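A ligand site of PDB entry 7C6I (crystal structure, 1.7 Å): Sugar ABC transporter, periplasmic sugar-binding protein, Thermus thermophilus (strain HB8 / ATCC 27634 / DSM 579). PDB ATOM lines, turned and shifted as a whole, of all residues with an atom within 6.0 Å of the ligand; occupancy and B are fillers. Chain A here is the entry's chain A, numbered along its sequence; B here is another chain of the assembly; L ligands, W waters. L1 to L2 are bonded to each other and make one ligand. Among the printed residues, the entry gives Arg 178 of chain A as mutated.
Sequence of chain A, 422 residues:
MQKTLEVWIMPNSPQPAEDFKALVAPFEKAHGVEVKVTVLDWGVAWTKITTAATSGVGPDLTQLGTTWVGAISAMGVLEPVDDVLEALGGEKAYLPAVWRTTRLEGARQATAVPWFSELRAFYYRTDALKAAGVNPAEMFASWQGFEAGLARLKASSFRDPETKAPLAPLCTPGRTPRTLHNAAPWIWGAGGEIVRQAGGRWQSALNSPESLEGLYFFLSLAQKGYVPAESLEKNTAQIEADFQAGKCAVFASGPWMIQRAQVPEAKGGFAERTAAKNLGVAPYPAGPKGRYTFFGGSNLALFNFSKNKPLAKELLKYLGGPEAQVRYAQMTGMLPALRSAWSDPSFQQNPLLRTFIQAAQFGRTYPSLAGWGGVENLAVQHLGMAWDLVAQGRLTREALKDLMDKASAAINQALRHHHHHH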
ATOM      1  N   TRP A  42     -16.144 -10.123  19.152  1.00  0.00           N
ATOM      2  CA  TRP A  42     -15.091  -9.317  18.510  1.00  0.00           C
ATOM      3  C   TRP A  42     -13.809 -10.125  18.310  1.00  0.00           C
ATOM      4  O   TRP A  42     -13.111  -9.867  17.357  1.00  0.00           O
ATOM      5  CB  TRP A  42     -14.783  -8.042  19.305  1.00  0.00           C
ATOM      6  CG  TRP A  42     -15.691  -6.896  18.967  1.00  0.00           C
ATOM      7  CD1 TRP A  42     -16.722  -6.409  19.704  1.00  0.00           C
ATOM      8  CD2 TRP A  42     -15.606  -6.086  17.779  1.00  0.00           C
ATOM      9  NE1 TRP A  42     -17.279  -5.345  19.061  1.00  0.00           N
ATOM     10  CE2 TRP A  42     -16.617  -5.113  17.892  1.00  0.00           C
ATOM     11  CE3 TRP A  42     -14.746  -6.027  16.700  1.00  0.00           C
ATOM     12  CZ2 TRP A  42     -16.841  -4.166  16.911  1.00  0.00           C
ATOM     13  CZ3 TRP A  42     -15.002  -5.114  15.701  1.00  0.00           C
ATOM     14  CH2 TRP A  42     -16.020  -4.159  15.823  1.00  0.00           C
ATOM     15  N   LEU A  64     -17.994  -4.439   9.916  1.00  0.00           N
ATOM     16  CA  LEU A  64     -16.531  -4.419   9.909  1.00  0.00           C
ATOM     17  C   LEU A  64     -16.121  -3.309  10.848  1.00  0.00           C
ATOM     18  O   LEU A  64     -16.700  -2.225  10.760  1.00  0.00           O
ATOM     19  CB  LEU A  64     -15.963  -4.089   8.550  1.00  0.00           C
ATOM     20  CG  LEU A  64     -16.353  -4.984   7.370  1.00  0.00           C
ATOM     21  CD1 LEU A  64     -15.853  -4.381   6.082  1.00  0.00           C
ATOM     22  CD2 LEU A  64     -15.762  -6.366   7.557  1.00  0.00           C
ATOM     23  N   GLY A  65     -15.118  -3.588  11.693  1.00  0.00           N
ATOM     24  CA  GLY A  65     -14.464  -2.468  12.344  1.00  0.00           C
ATOM     25  C   GLY A  65     -13.914  -1.530  11.295  1.00  0.00           C
ATOM     26  O   GLY A  65     -13.458  -1.999  10.220  1.00  0.00           O
ATOM     27  N   THR A  66     -13.902  -0.218  11.566  1.00  0.00           N
ATOM     28  CA  THR A  66     -13.334   0.747  10.614  1.00  0.00           C
ATOM     29  C   THR A  66     -11.927   0.348  10.166  1.00  0.00           C
ATOM     30  O   THR A  66     -11.560   0.557   8.973  1.00  0.00           O
ATOM     31  CB  THR A  66     -13.335   2.181  11.137  1.00  0.00           C
ATOM     32  OG1 THR A  66     -12.657   2.174  12.390  1.00  0.00           O
ATOM     33  CG2 THR A  66     -14.743   2.717  11.125  1.00  0.00           C
ATOM     34  N   THR A  67     -11.108  -0.202  11.060  1.00  0.00           N
ATOM     35  CA  THR A  67      -9.699  -0.540  10.796  1.00  0.00           C
ATOM     36  C   THR A  67      -9.593  -1.836   9.987  1.00  0.00           C
ATOM     37  O   THR A  67      -8.439  -2.185   9.636  1.00  0.00           O
ATOM     38  CB  THR A  67      -8.902  -0.625  12.109  1.00  0.00           C
ATOM     39  OG1 THR A  67      -9.324  -1.762  12.850  1.00  0.00           O
ATOM     40  CG2 THR A  67      -9.022   0.651  12.919  1.00  0.00           C
ATOM     41  N   TRP A  68     -10.696  -2.523   9.698  1.00  0.00           N
ATOM     42  CA  TRP A  68     -10.699  -3.761   8.891  1.00  0.00           C
ATOM     43  C   TRP A  68     -11.027  -3.517   7.417  1.00  0.00           C
ATOM     44  O   TRP A  68     -10.962  -4.445   6.574  1.00  0.00           O
ATOM     45  CB  TRP A  68     -11.748  -4.709   9.477  1.00  0.00           C
ATOM     46  CG  TRP A  68     -11.448  -5.245  10.845  1.00  0.00           C
ATOM     47  CD1 TRP A  68     -10.380  -4.951  11.647  1.00  0.00           C
ATOM     48  CD2 TRP A  68     -12.285  -6.140  11.586  1.00  0.00           C
ATOM     49  NE1 TRP A  68     -10.524  -5.588  12.852  1.00  0.00           N
ATOM     50  CE2 TRP A  68     -11.655  -6.342  12.838  1.00  0.00           C
ATOM     51  CE3 TRP A  68     -13.508  -6.782  11.350  1.00  0.00           C
ATOM     52  CZ2 TRP A  68     -12.223  -7.172  13.803  1.00  0.00           C
ATOM     53  CZ3 TRP A  68     -14.073  -7.569  12.331  1.00  0.00           C
ATOM     54  CH2 TRP A  68     -13.408  -7.791  13.517  1.00  0.00           C
ATOM     55  N   PHE A 116     -21.614   3.322  12.846  1.00  0.00           N
ATOM     56  CA  PHE A 116     -21.530   4.106  14.079  1.00  0.00           C
ATOM     57  C   PHE A 116     -20.092   4.400  14.385  1.00  0.00           C
ATOM     58  O   PHE A 116     -19.166   3.679  13.914  1.00  0.00           O
ATOM     59  CB  PHE A 116     -22.243   3.416  15.246  1.00  0.00           C
ATOM     60  CG  PHE A 116     -21.677   2.084  15.681  1.00  0.00           C
ATOM     61  CD1 PHE A 116     -20.574   1.999  16.512  1.00  0.00           C
ATOM     62  CD2 PHE A 116     -22.209   0.895  15.204  1.00  0.00           C
ATOM     63  CE1 PHE A 116     -20.046   0.783  16.918  1.00  0.00           C
ATOM     64  CE2 PHE A 116     -21.704  -0.308  15.627  1.00  0.00           C
ATOM     65  CZ  PHE A 116     -20.590  -0.381  16.407  1.00  0.00           C
ATOM     66  N   GLU A 118     -17.053   5.361  17.232  1.00  0.00           N
ATOM     67  CA  GLU A 118     -16.393   5.333  18.544  1.00  0.00           C
ATOM     68  C   GLU A 118     -15.482   6.578  18.559  1.00  0.00           C
ATOM     69  O   GLU A 118     -14.688   6.797  17.599  1.00  0.00           O
ATOM     70  CB  GLU A 118     -15.639   4.031  18.762  1.00  0.00           C
ATOM     71  CG  GLU A 118     -14.923   4.072  20.054  1.00  0.00           C
ATOM     72  CD  GLU A 118     -14.140   2.835  20.473  1.00  0.00           C
ATOM     73  OE1 GLU A 118     -14.304   1.729  19.817  1.00  0.00           O
ATOM     74  OE2 GLU A 118     -13.391   2.994  21.491  1.00  0.00           O
ATOM     75  N   ARG A 178      -5.738  -2.477  22.777  1.00  0.00           N
ATOM     76  CA  ARG A 178      -6.215  -1.221  22.175  1.00  0.00           C
ATOM     77  C   ARG A 178      -5.310  -0.040  22.538  1.00  0.00           C
ATOM     78  O   ARG A 178      -5.691   1.144  22.410  1.00  0.00           O
ATOM     79  CB  ARG A 178      -7.672  -0.997  22.554  1.00  0.00           C
ATOM     80  CG  ARG A 178      -8.542  -2.106  22.003  1.00  0.00           C
ATOM     81  CD  ARG A 178      -9.989  -1.720  22.198  1.00  0.00           C
ATOM     82  NE  ARG A 178     -10.507  -2.099  23.498  1.00  0.00           N
ATOM     83  CZ  ARG A 178     -11.614  -1.576  24.027  1.00  0.00           C
ATOM     84  NH1 ARG A 178     -12.279  -0.647  23.381  1.00  0.00           N
ATOM     85  NH2 ARG A 178     -12.094  -2.039  25.179  1.00  0.00           N
ATOM     86  N   HIS A 181      -4.866   3.165  20.133  1.00  0.00           N
ATOM     87  CA  HIS A 181      -5.927   4.179  20.068  1.00  0.00           C
ATOM     88  C   HIS A 181      -5.701   5.221  21.187  1.00  0.00           C
ATOM     89  O   HIS A 181      -5.981   6.393  20.963  1.00  0.00           O
ATOM     90  CB  HIS A 181      -7.323   3.578  20.234  1.00  0.00           C
ATOM     91  CG  HIS A 181      -7.591   2.374  19.432  1.00  0.00           C
ATOM     92  ND1 HIS A 181      -6.919   2.076  18.250  1.00  0.00           N
ATOM     93  CD2 HIS A 181      -8.570   1.442  19.547  1.00  0.00           C
ATOM     94  CE1 HIS A 181      -7.423   0.955  17.750  1.00  0.00           C
ATOM     95  NE2 HIS A 181      -8.448   0.558  18.530  1.00  0.00           N
ATOM     96  N   TRP A 256     -20.755   6.552  25.895  1.00  0.00           N
ATOM     97  CA  TRP A 256     -21.529   5.566  26.693  1.00  0.00           C
ATOM     98  C   TRP A 256     -21.470   5.886  28.194  1.00  0.00           C
ATOM     99  O   TRP A 256     -22.418   5.490  28.909  1.00  0.00           O
ATOM    100  CB  TRP A 256     -21.049   4.141  26.452  1.00  0.00           C
ATOM    101  CG  TRP A 256     -19.572   3.939  26.568  1.00  0.00           C
ATOM    102  CD1 TRP A 256     -18.851   3.650  27.706  1.00  0.00           C
ATOM    103  CD2 TRP A 256     -18.593   4.005  25.507  1.00  0.00           C
ATOM    104  NE1 TRP A 256     -17.533   3.508  27.416  1.00  0.00           N
ATOM    105  CE2 TRP A 256     -17.338   3.709  26.078  1.00  0.00           C
ATOM    106  CE3 TRP A 256     -18.656   4.181  24.127  1.00  0.00           C
ATOM    107  CZ2 TRP A 256     -16.168   3.678  25.324  1.00  0.00           C
ATOM    108  CZ3 TRP A 256     -17.508   4.111  23.384  1.00  0.00           C
ATOM    109  CH2 TRP A 256     -16.271   3.898  23.969  1.00  0.00           C
ATOM    110  N   PHE A 294      -9.336  10.745  18.542  1.00  0.00           N
ATOM    111  CA  PHE A 294      -9.359   9.396  17.931  1.00  0.00           C
ATOM    112  C   PHE A 294     -10.782   8.993  17.515  1.00  0.00           C
ATOM    113  O   PHE A 294     -11.722   9.039  18.389  1.00  0.00           O
ATOM    114  CB  PHE A 294      -8.826   8.368  18.918  1.00  0.00           C
ATOM    115  CG  PHE A 294      -8.887   6.984  18.345  1.00  0.00           C
ATOM    116  CD1 PHE A 294      -7.936   6.605  17.418  1.00  0.00           C
ATOM    117  CD2 PHE A 294      -9.953   6.126  18.613  1.00  0.00           C
ATOM    118  CE1 PHE A 294      -7.999   5.366  16.807  1.00  0.00           C
ATOM    119  CE2 PHE A 294      -9.997   4.872  18.028  1.00  0.00           C
ATOM    120  CZ  PHE A 294      -8.999   4.491  17.141  1.00  0.00           C
ATOM    121  N   PHE A 295     -10.939   8.524  16.295  1.00  0.00           N
ATOM    122  CA  PHE A 295     -12.187   7.923  15.756  1.00  0.00           C
ATOM    123  C   PHE A 295     -11.935   6.469  15.382  1.00  0.00           C
ATOM    124  O   PHE A 295     -10.966   6.122  14.646  1.00  0.00           O
ATOM    125  CB  PHE A 295     -12.727   8.638  14.530  1.00  0.00           C
ATOM    126  CG  PHE A 295     -13.820   9.612  14.844  1.00  0.00           C
ATOM    127  CD1 PHE A 295     -13.571  10.718  15.667  1.00  0.00           C
ATOM    128  CD2 PHE A 295     -15.095   9.420  14.329  1.00  0.00           C
ATOM    129  CE1 PHE A 295     -14.579  11.608  15.951  1.00  0.00           C
ATOM    130  CE2 PHE A 295     -16.113  10.305  14.649  1.00  0.00           C
ATOM    131  CZ  PHE A 295     -15.856  11.354  15.489  1.00  0.00           C
ATOM    132  N   GLY A 296     -12.846   5.661  15.800  1.00  0.00           N
ATOM    133  CA  GLY A 296     -13.053   4.290  15.269  1.00  0.00           C
ATOM    134  C   GLY A 296     -14.528   4.078  15.098  1.00  0.00           C
ATOM    135  O   GLY A 296     -15.270   5.023  14.751  1.00  0.00           O
ATOM    136  N   GLY A 297     -14.962   2.854  15.377  1.00  0.00           N
ATOM    137  CA  GLY A 297     -16.338   2.462  15.144  1.00  0.00           C
ATOM    138  C   GLY A 297     -16.449   1.358  14.125  1.00  0.00           C
ATOM    139  O   GLY A 297     -15.465   0.607  13.887  1.00  0.00           O
ATOM    140  N   SER A 298     -17.614   1.229  13.545  1.00  0.00           N
ATOM    141  CA  SER A 298     -17.940   0.126  12.628  1.00  0.00           C
ATOM    142  C   SER A 298     -18.729   0.633  11.413  1.00  0.00           C
ATOM    143  O   SER A 298     -19.511   1.572  11.524  1.00  0.00           O
ATOM    144  CB  SER A 298     -18.695  -0.992  13.356  1.00  0.00           C
ATOM    145  OG  SER A 298     -17.856  -1.703  14.249  1.00  0.00           O
ATOM    146  N   MET A 334     -22.956   4.719  21.305  1.00  0.00           N
ATOM    147  CA  MET A 334     -21.963   5.354  20.376  1.00  0.00           C
ATOM    148  C   MET A 334     -22.510   6.634  19.749  1.00  0.00           C
ATOM    149  O   MET A 334     -23.644   7.090  20.064  1.00  0.00           O
ATOM    150  CB  MET A 334     -21.694   4.311  19.290  1.00  0.00           C
ATOM    151  CG  MET A 334     -21.037   3.071  19.777  1.00  0.00           C
ATOM    152  SD  MET A 334     -19.240   3.313  20.067  1.00  0.00           S
ATOM    153  CE  MET A 334     -18.894   1.861  21.041  1.00  0.00           C
ATOM    154  N   GLU A 376      -0.865  -2.546  13.274  1.00  0.00           N
ATOM    155  CA  GLU A 376      -1.420  -2.339  14.626  1.00  0.00           C
ATOM    156  C   GLU A 376      -0.875  -3.405  15.571  1.00  0.00           C
ATOM    157  O   GLU A 376      -0.470  -3.058  16.683  1.00  0.00           O
ATOM    158  CB  GLU A 376      -2.939  -2.279  14.572  1.00  0.00           C
ATOM    159  CG  GLU A 376      -3.508  -1.892  15.916  1.00  0.00           C
ATOM    160  CD  GLU A 376      -5.009  -1.592  15.961  1.00  0.00           C
ATOM    161  OE1 GLU A 376      -5.613  -1.275  14.917  1.00  0.00           O
ATOM    162  OE2 GLU A 376      -5.552  -1.659  17.064  1.00  0.00           O
ATOM    163  N   LYS B  92      -2.848 -10.444  11.098  1.00  0.00           N
ATOM    164  CA  LYS B  92      -3.651  -9.957  12.223  1.00  0.00           C
ATOM    165  C   LYS B  92      -4.073 -11.105  13.139  1.00  0.00           C
ATOM    166  O   LYS B  92      -4.088 -10.833  14.302  1.00  0.00           O
ATOM    167  CB  LYS B  92      -4.898  -9.249  11.687  1.00  0.00           C
ATOM    168  CG  LYS B  92      -6.083  -9.202  12.610  1.00  0.00           C
ATOM    169  CD  LYS B  92      -6.983  -8.007  12.323  1.00  0.00           C
ATOM    170  CE  LYS B  92      -8.118  -7.986  13.327  1.00  0.00           C
ATOM    171  NZ  LYS B  92      -7.612  -7.675  14.692  1.00  0.00           N
HETATM  172  C1  LIG L   1     -14.293  -2.413  19.784  1.00  0.00           C
HETATM  173  C2  LIG L   1     -14.872  -1.730  21.014  1.00  0.00           C
HETATM  174  C3  LIG L   1     -15.609  -2.731  21.955  1.00  0.00           C
HETATM  175  C4  LIG L   1     -14.726  -3.942  22.207  1.00  0.00           C
HETATM  176  C5  LIG L   1     -15.252  -5.129  23.033  1.00  0.00           C
HETATM  177  C6  LIG L   1     -13.391  -3.384  20.503  1.00  0.00           C
HETATM  178  O1  LIG L   1     -12.145  -3.720  19.913  1.00  0.00           O
HETATM  179  O2  LIG L   1     -13.615  -1.386  19.006  1.00  0.00           O
HETATM  180  O3  LIG L   1     -15.663  -0.584  20.724  1.00  0.00           O
HETATM  181  O4  LIG L   1     -15.796  -2.020  23.167  1.00  0.00           O
HETATM  182  O5  LIG L   1     -14.267  -4.458  20.967  1.00  0.00           O
HETATM  183  O6  LIG L   1     -14.230  -6.140  22.812  1.00  0.00           O
HETATM  184  C1  LG2 L   2     -13.258  -0.230  16.982  1.00  0.00           C
HETATM  185  C2  LG2 L   2     -12.927  -0.290  15.512  1.00  0.00           C
HETATM  186  C3  LG2 L   2     -11.883  -1.341  15.229  1.00  0.00           C
HETATM  187  C4  LG2 L   2     -12.343  -2.621  15.910  1.00  0.00           C
HETATM  188  C5  LG2 L   2     -11.349  -3.777  15.674  1.00  0.00           C
HETATM  189  C6  LG2 L   2     -13.618  -1.577  17.605  1.00  0.00           C
HETATM  190  O1  LG2 L   2     -14.282   0.771  17.139  1.00  0.00           O
HETATM  191  O2  LG2 L   2     -12.467   1.018  15.064  1.00  0.00           O
HETATM  192  O3  LG2 L   2     -11.789  -1.478  13.828  1.00  0.00           O
HETATM  193  O4  LG2 L   2     -12.546  -2.455  17.317  1.00  0.00           O
HETATM  194  O5  LG2 L   2     -10.107  -3.621  16.343  1.00  0.00           O
HETATM  195  O   HOH W   1      -7.625  -2.771  18.306  1.00  0.00           O
HETATM  196  O   HOH W   2     -10.570  -5.167  18.795  1.00  0.00           O
HETATM  197  O   HOH W   3     -16.926  -0.479  16.471  1.00  0.00           O
HETATM  198  O   HOH W   4     -10.055  -1.586  18.781  1.00  0.00           O
HETATM  199  O   HOH W   5     -17.720  -0.948  18.932  1.00  0.00           O
HETATM  200  O   HOH W   6      -8.417  -5.305  15.000  1.00  0.00           O
HETATM  201  O   HOH W   7     -12.540  -5.458  25.302  1.00  0.00           O
HETATM  202  O   HOH W   8      -8.206  -1.447  15.244  1.00  0.00           O
HETATM  203  O   HOH W   9     -11.809   0.487  20.645  1.00  0.00           O
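O of Glu 118 lies within hydrogen-bond range of N of Gly 296 (2.8 Å).
The backbone NH of Thr 66 lies within hydrogen-bond range of the backbone carbonyl oxygen of Gly 297, 2.9 Å away.
An oxygen (O1) of LG2 L2 sits at hydrogen-bond distance from the backbone NH (N) of Gly 297, 2.8 Å away.
An oxygen (O3) of LG2 L2 is in hydrogen-bond range of the backbone NH of Thr 66 (3.3 Å).
O3 of LG2 L2 sits at hydrogen-bond distance from N of Thr 67, at 3.1 Å.
The side-chain carboxylate of Glu 118 lies within hydrogen-bond range of an oxygen (O3) of LIG L1, at 2.8 Å.
An oxygen (O3) of LG2 L2 lies within hydrogen-bond range of the side-chain hydroxyl (OG1) of Thr 67 (2.7 Å).
O2 of LG2 L2 sits at hydrogen-bond distance from OG1 of Thr 66 (2.9 Å).
An oxygen (O2) of LG2 L2 sits close to the backbone carbonyl oxygen (O) of Gly 297 (3.2 Å).
CD1 of Trp 42 touches O5 of LIG L1 (3.4 Å).
CA of Gly 65 touches O3 of LG2 L2, 3.2 Å away.
NE1 of Trp 68 touches C5 of LG2 L2 (3.5 Å).
NH1 of Arg 178 touches C2 of LIG L1, at 3.7 Å.
CA of Gly 296 touches O2 of LG2 L2 (3.3 Å).
Within 4 Å of the ligand: Trp 42, Gly 65, Thr 66, Thr 67, Trp 68, Glu 118, Arg 178, Gly 296 and Gly 297.
Water W6 lies within hydrogen-bond range of NZ of Lys 92 of chain B (2.5 Å), O5 of LG2 L2 (2.7 Å) and NE1 of Trp 68 (3.0 Å).
Water W3 lies within hydrogen-bond range of the side-chain hydroxyl (OG) of Ser 298 (2.7 Å), an oxygen (O1) of LG2 L2 (3.0 Å) and the backbone carbonyl oxygen (O) of Gly 297 (3.2 Å).
Water W9 lies within hydrogen-bond range of OE1 of Glu 118, NH1 of Arg 178 and O2 of LIG L1.
Water W7 lies within hydrogen-bond range of O6 of LIG L1 (3.1 Å) and NH2 of Arg 178 (3.5 Å).
Water W8 lies within hydrogen-bond range of the side-chain carboxylate of Glu 376 (2.6 Å), the side-chain hydroxyl of Thr 67 (2.7 Å) and an oxygen (O5) of LG2 L2 (3.1 Å).
Water W1 lies within hydrogen-bond range of the side-chain carboxylate (OE2) of Glu 376 (2.7 Å), an oxygen (O5) of LG2 L2 (3.3 Å) and a ring nitrogen (NE2) of His 181 (3.4 Å).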
